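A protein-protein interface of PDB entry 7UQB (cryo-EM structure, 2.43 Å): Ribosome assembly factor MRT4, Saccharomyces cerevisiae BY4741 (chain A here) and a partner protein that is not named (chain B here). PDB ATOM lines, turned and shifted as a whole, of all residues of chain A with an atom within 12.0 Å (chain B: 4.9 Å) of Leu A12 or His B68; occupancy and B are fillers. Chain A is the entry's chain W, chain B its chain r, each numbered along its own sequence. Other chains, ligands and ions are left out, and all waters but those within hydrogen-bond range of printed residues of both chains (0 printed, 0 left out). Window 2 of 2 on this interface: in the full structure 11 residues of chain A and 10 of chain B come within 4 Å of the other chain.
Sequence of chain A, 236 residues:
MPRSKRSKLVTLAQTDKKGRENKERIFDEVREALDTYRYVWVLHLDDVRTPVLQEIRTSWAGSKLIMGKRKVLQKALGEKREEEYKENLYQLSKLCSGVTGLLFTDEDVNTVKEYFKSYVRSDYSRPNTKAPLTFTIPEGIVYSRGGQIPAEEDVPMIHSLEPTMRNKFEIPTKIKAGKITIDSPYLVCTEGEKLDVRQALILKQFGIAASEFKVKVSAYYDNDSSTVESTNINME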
ATOM      1  N   LYS A   8      -7.287 -12.843  30.563  1.00  0.00           N
ATOM      2  CA  LYS A   8      -7.588 -14.139  31.157  1.00  0.00           C
ATOM      3  C   LYS A   8      -6.311 -14.931  31.411  1.00  0.00           C
ATOM      4  O   LYS A   8      -5.411 -14.977  30.569  1.00  0.00           O
ATOM      5  CB  LYS A   8      -8.518 -14.940  30.247  1.00  0.00           C
ATOM      6  CG  LYS A   8      -9.799 -14.219  29.864  1.00  0.00           C
ATOM      7  CD  LYS A   8     -10.633 -15.052  28.902  1.00  0.00           C
ATOM      8  CE  LYS A   8     -11.131 -16.331  29.556  1.00  0.00           C
ATOM      9  NZ  LYS A   8     -12.023 -16.051  30.715  1.00  0.00           N
ATOM     10  N   LEU A   9      -6.238 -15.556  32.581  1.00  0.00           N
ATOM     11  CA  LEU A   9      -5.123 -16.441  32.886  1.00  0.00           C
ATOM     12  C   LEU A   9      -5.211 -17.704  32.038  1.00  0.00           C
ATOM     13  O   LEU A   9      -6.293 -18.262  31.834  1.00  0.00           O
ATOM     14  CB  LEU A   9      -5.115 -16.796  34.370  1.00  0.00           C
ATOM     15  CG  LEU A   9      -5.101 -15.612  35.340  1.00  0.00           C
ATOM     16  CD1 LEU A   9      -5.063 -16.093  36.782  1.00  0.00           C
ATOM     17  CD2 LEU A   9      -3.930 -14.685  35.047  1.00  0.00           C
ATOM     18  N   VAL A  10      -4.063 -18.150  31.539  1.00  0.00           N
ATOM     19  CA  VAL A  10      -3.982 -19.275  30.615  1.00  0.00           C
ATOM     20  C   VAL A  10      -3.375 -20.462  31.346  1.00  0.00           C
ATOM     21  O   VAL A  10      -2.317 -20.340  31.975  1.00  0.00           O
ATOM     22  CB  VAL A  10      -3.161 -18.916  29.364  1.00  0.00           C
ATOM     23  CG1 VAL A  10      -3.074 -20.106  28.420  1.00  0.00           C
ATOM     24  CG2 VAL A  10      -3.764 -17.712  28.661  1.00  0.00           C
ATOM     25  N   THR A  11      -4.048 -21.605  31.268  1.00  0.00           N
ATOM     26  CA  THR A  11      -3.569 -22.854  31.839  1.00  0.00           C
ATOM     27  C   THR A  11      -3.376 -23.876  30.729  1.00  0.00           C
ATOM     28  O   THR A  11      -4.063 -23.839  29.705  1.00  0.00           O
ATOM     29  CB  THR A  11      -4.548 -23.411  32.872  1.00  0.00           C
ATOM     30  OG1 THR A  11      -5.775 -23.755  32.216  1.00  0.00           O
ATOM     31  CG2 THR A  11      -4.831 -22.381  33.954  1.00  0.00           C
ATOM     32  N   LEU A  12      -2.438 -24.793  30.941  1.00  0.00           N
ATOM     33  CA  LEU A  12      -2.159 -25.871  29.997  1.00  0.00           C
ATOM     34  C   LEU A  12      -2.366 -27.191  30.731  1.00  0.00           C
ATOM     35  O   LEU A  12      -1.417 -27.783  31.247  1.00  0.00           O
ATOM     36  CB  LEU A  12      -0.752 -25.752  29.428  1.00  0.00           C
ATOM     37  CG  LEU A  12      -0.500 -24.502  28.586  1.00  0.00           C
ATOM     38  CD1 LEU A  12       0.880 -24.542  27.952  1.00  0.00           C
ATOM     39  CD2 LEU A  12      -1.575 -24.369  27.528  1.00  0.00           C
ATOM     40  N   ALA A  13      -3.612 -27.656  30.759  1.00  0.00           N
ATOM     41  CA  ALA A  13      -3.989 -28.875  31.456  1.00  0.00           C
ATOM     42  C   ALA A  13      -4.692 -29.812  30.480  1.00  0.00           C
ATOM     43  O   ALA A  13      -4.956 -29.458  29.327  1.00  0.00           O
ATOM     44  CB  ALA A  13      -4.879 -28.567  32.665  1.00  0.00           C
ATOM     45  N   GLN A  14      -5.003 -31.018  30.953  1.00  0.00           N
ATOM     46  CA  GLN A  14      -5.565 -32.047  30.086  1.00  0.00           C
ATOM     47  C   GLN A  14      -7.084 -31.985  29.999  1.00  0.00           C
ATOM     48  O   GLN A  14      -7.649 -32.215  28.925  1.00  0.00           O
ATOM     49  CB  GLN A  14      -5.141 -33.433  30.575  1.00  0.00           C
ATOM     50  CG  GLN A  14      -3.668 -33.555  30.921  1.00  0.00           C
ATOM     51  CD  GLN A  14      -2.762 -33.333  29.727  1.00  0.00           C
ATOM     52  OE1 GLN A  14      -3.112 -33.663  28.594  1.00  0.00           O
ATOM     53  NE2 GLN A  14      -1.589 -32.769  29.976  1.00  0.00           N
ATOM     54  N   THR A  15      -7.760 -31.677  31.101  1.00  0.00           N
ATOM     55  CA  THR A  15      -9.214 -31.748  31.133  1.00  0.00           C
ATOM     56  C   THR A  15      -9.822 -30.482  30.540  1.00  0.00           C
ATOM     57  O   THR A  15      -9.542 -29.371  31.000  1.00  0.00           O
ATOM     58  CB  THR A  15      -9.711 -31.955  32.563  1.00  0.00           C
ATOM     59  OG1 THR A  15      -8.928 -32.972  33.197  1.00  0.00           O
ATOM     60  CG2 THR A  15     -11.168 -32.386  32.558  1.00  0.00           C
ATOM     61  N   ASP A  16     -10.652 -30.656  29.519  1.00  0.00           N
ATOM     62  CA  ASP A  16     -11.345 -29.558  28.863  1.00  0.00           C
ATOM     63  C   ASP A  16     -12.788 -29.482  29.350  1.00  0.00           C
ATOM     64  O   ASP A  16     -13.320 -30.420  29.948  1.00  0.00           O
ATOM     65  CB  ASP A  16     -11.290 -29.727  27.342  1.00  0.00           C
ATOM     66  CG  ASP A  16      -9.867 -29.748  26.811  1.00  0.00           C
ATOM     67  OD1 ASP A  16      -9.058 -28.899  27.241  1.00  0.00           O
ATOM     68  OD2 ASP A  16      -9.554 -30.620  25.974  1.00  0.00           O
ATOM     69  N   LYS A  17     -13.421 -28.343  29.083  1.00  0.00           N
ATOM     70  CA  LYS A  17     -14.763 -28.092  29.594  1.00  0.00           C
ATOM     71  C   LYS A  17     -15.797 -28.965  28.897  1.00  0.00           C
ATOM     72  O   LYS A  17     -15.659 -29.325  27.725  1.00  0.00           O
ATOM     73  CB  LYS A  17     -15.139 -26.623  29.423  1.00  0.00           C
ATOM     74  CG  LYS A  17     -14.391 -25.685  30.346  1.00  0.00           C
ATOM     75  CD  LYS A  17     -14.918 -24.267  30.232  1.00  0.00           C
ATOM     76  CE  LYS A  17     -14.157 -23.330  31.150  1.00  0.00           C
ATOM     77  NZ  LYS A  17     -14.674 -21.939  31.077  1.00  0.00           N
ATOM     78  N   LYS B  64       4.188 -22.298  22.388  1.00  0.00           N
ATOM     79  CA  LYS B  64       3.932 -23.199  23.513  1.00  0.00           C
ATOM     80  C   LYS B  64       2.472 -23.647  23.555  1.00  0.00           C
ATOM     81  O   LYS B  64       2.186 -24.825  23.812  1.00  0.00           O
ATOM     82  CB  LYS B  64       4.329 -22.526  24.826  1.00  0.00           C
ATOM     83  CG  LYS B  64       4.197 -23.425  26.045  1.00  0.00           C
ATOM     84  CD  LYS B  64       4.702 -22.735  27.299  1.00  0.00           C
ATOM     85  CE  LYS B  64       6.174 -22.374  27.173  1.00  0.00           C
ATOM     86  NZ  LYS B  64       6.670 -21.646  28.373  1.00  0.00           N
ATOM     87  N   ILE B  65       1.539 -22.724  23.300  1.00  0.00           N
ATOM     88  CA  ILE B  65       0.123 -23.091  23.247  1.00  0.00           C
ATOM     89  C   ILE B  65      -0.128 -24.079  22.112  1.00  0.00           C
ATOM     90  O   ILE B  65      -0.866 -25.063  22.273  1.00  0.00           O
ATOM     91  CB  ILE B  65      -0.760 -21.836  23.100  1.00  0.00           C
ATOM     92  CG1 ILE B  65      -0.518 -20.852  24.245  1.00  0.00           C
ATOM     93  CG2 ILE B  65      -2.230 -22.219  23.034  1.00  0.00           C
ATOM     94  CD1 ILE B  65      -0.692 -21.436  25.612  1.00  0.00           C
ATOM     95  N   LYS B  66       0.479 -23.827  20.947  1.00  0.00           N
ATOM     96  CA  LYS B  66       0.331 -24.728  19.809  1.00  0.00           C
ATOM     97  C   LYS B  66       0.864 -26.117  20.130  1.00  0.00           C
ATOM     98  O   LYS B  66       0.241 -27.123  19.776  1.00  0.00           O
ATOM     99  CB  LYS B  66       1.050 -24.145  18.592  1.00  0.00           C
ATOM    100  CG  LYS B  66       1.110 -25.066  17.381  1.00  0.00           C
ATOM    101  CD  LYS B  66      -0.242 -25.178  16.697  1.00  0.00           C
ATOM    102  CE  LYS B  66      -0.170 -26.078  15.472  1.00  0.00           C
ATOM    103  NZ  LYS B  66      -1.465 -26.125  14.738  1.00  0.00           N
ATOM    104  N   ALA B  67       2.014 -26.189  20.805  1.00  0.00           N
ATOM    105  CA  ALA B  67       2.588 -27.480  21.169  1.00  0.00           C
ATOM    106  C   ALA B  67       1.698 -28.230  22.152  1.00  0.00           C
ATOM    107  O   ALA B  67       1.509 -29.445  22.021  1.00  0.00           O
ATOM    108  CB  ALA B  67       3.986 -27.287  21.756  1.00  0.00           C
ATOM    109  N   HIS B  68       1.148 -27.525  23.146  1.00  0.00           N
ATOM    110  CA  HIS B  68       0.259 -28.182  24.102  1.00  0.00           C
ATOM    111  C   HIS B  68      -0.995 -28.719  23.419  1.00  0.00           C
ATOM    112  O   HIS B  68      -1.404 -29.861  23.668  1.00  0.00           O
ATOM    113  CB  HIS B  68      -0.118 -27.218  25.227  1.00  0.00           C
ATOM    114  CG  HIS B  68      -1.062 -27.803  26.230  1.00  0.00           C
ATOM    115  ND1 HIS B  68      -0.669 -28.734  27.167  1.00  0.00           N
ATOM    116  CD2 HIS B  68      -2.384 -27.595  26.439  1.00  0.00           C
ATOM    117  CE1 HIS B  68      -1.706 -29.072  27.911  1.00  0.00           C
ATOM    118  NE2 HIS B  68      -2.759 -28.394  27.491  1.00  0.00           N
ATOM    119  N   GLU B  69      -1.608 -27.921  22.541  1.00  0.00           N
ATOM    120  CA  GLU B  69      -2.806 -28.386  21.844  1.00  0.00           C
ATOM    121  C   GLU B  69      -2.487 -29.534  20.891  1.00  0.00           C
ATOM    122  O   GLU B  69      -3.288 -30.463  20.740  1.00  0.00           O
ATOM    123  CB  GLU B  69      -3.467 -27.232  21.092  1.00  0.00           C
ATOM    124  CG  GLU B  69      -3.976 -26.115  21.989  1.00  0.00           C
ATOM    125  CD  GLU B  69      -5.089 -26.560  22.922  1.00  0.00           C
ATOM    126  OE1 GLU B  69      -5.871 -27.459  22.544  1.00  0.00           O
ATOM    127  OE2 GLU B  69      -5.183 -26.008  24.038  1.00  0.00           O
ATOM    128  N   GLN B  70      -1.319 -29.491  20.242  1.00  0.00           N
ATOM    129  CA  GLN B  70      -0.926 -30.566  19.339  1.00  0.00           C
ATOM    130  C   GLN B  70      -0.645 -31.857  20.094  1.00  0.00           C
ATOM    131  O   GLN B  70      -0.900 -32.948  19.573  1.00  0.00           O
ATOM    132  CB  GLN B  70       0.298 -30.133  18.532  1.00  0.00           C
ATOM    133  CG  GLN B  70       0.597 -30.970  17.307  1.00  0.00           C
ATOM    134  CD  GLN B  70       1.693 -30.361  16.455  1.00  0.00           C
ATOM    135  OE1 GLN B  70       2.062 -29.202  16.639  1.00  0.00           O
ATOM    136  NE2 GLN B  70       2.221 -31.141  15.518  1.00  0.00           N
ATOM    137  N   SER B  71      -0.117 -31.757  21.315  1.00  0.00           N
ATOM    138  CA  SER B  71       0.056 -32.948  22.139  1.00  0.00           C
ATOM    139  C   SER B  71      -1.285 -33.472  22.639  1.00  0.00           C
ATOM    140  O   SER B  71      -1.472 -34.685  22.779  1.00  0.00           O
ATOM    141  CB  SER B  71       0.987 -32.642  23.312  1.00  0.00           C
ATOM    142  OG  SER B  71       1.324 -33.823  24.018  1.00  0.00           O
ATOM    143  N   LYS B  72      -2.229 -32.569  22.917  1.00  0.00           N
ATOM    144  CA  LYS B  72      -3.530 -32.975  23.439  1.00  0.00           C
ATOM    145  C   LYS B  72      -4.468 -33.506  22.360  1.00  0.00           C
ATOM    146  O   LYS B  72      -5.442 -34.191  22.691  1.00  0.00           O
ATOM    147  CB  LYS B  72      -4.184 -31.796  24.164  1.00  0.00           C
ATOM    148  CG  LYS B  72      -4.971 -32.179  25.401  1.00  0.00           C
ATOM    149  CD  LYS B  72      -5.241 -30.965  26.275  1.00  0.00           C
ATOM    150  CE  LYS B  72      -6.068 -29.925  25.540  1.00  0.00           C
ATOM    151  NZ  LYS B  72      -6.260 -28.695  26.356  1.00  0.00           N
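Of the 10 printed residues of chain A, 5 touch a printed residue of chain B.
Printed residues of chain A that touch a printed residue of chain B: Val A10, Leu A12, Ala A13, Gln A14 and Asp A16.
Of the 9 printed residues of chain B, 4 touch a printed residue of chain A.
Printed residues of chain B that touch a printed residue of chain A: Lys B64, Ile B65, His B68 and Lys B72.
Among the printed residues, 8 pairs touch across the chains.
Printed residues of chain B within 4 Å of Leu A12: Lys B64, Ile B65 and His B68.
His B68 touches just these residues of chain A: Leu A12 and Ala A13.
Ile B65 touches just these residues of chain A: Val A10 (3.9 Å) and Leu A12 (3.6 Å).
Glu B69 touches none of the printed residues of chain A.
Of chain A, only Ala A13, Gln A14 and Asp A16 come within 4 Å of Lys B72.
Printed residues of chain B within 4 Å of Ala A13: His B68 (3.1 Å) and Lys B72 (3.3 Å).
Printed residues of chain B within 4 Å of Val A10: Ile B65 (3.9 Å).
Printed residues of chain A within 4 Å of Lys B64: Leu A12 (3.99 Å).
Gln B70 touches none of the printed residues of chain A.
The nearest residue of chain A that does not touch His B68 is Gln A14 (4.2 Å).
The side-chain carboxylate (OD1) of Asp A16 is in salt-bridge range of the side-chain amino group (NZ) of Lys B72 (2.9 Å).
The backbone carbonyl oxygen (O) of Ala A13 sits at hydrogen-bond distance from the side-chain amino group (NZ) of Lys B72 (3.3 Å).
NE2 of His B68 lies within hydrogen-bond range of O of Ala A13 (3.1 Å).
OE2 of Glu B69 lies within salt-bridge range of NZ of Lys B72 (3.7 Å).
Among the printed residues, pairs that only touch across the chains: Val A10 with Ile B65 (3.9 Å), Leu A12 with Lys B64 (3.99 Å), Leu A12 with Ile B65 (3.6 Å), Leu A12 with His B68 (3.5 Å) and Gln A14 with Lys B72 (3.8 Å).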
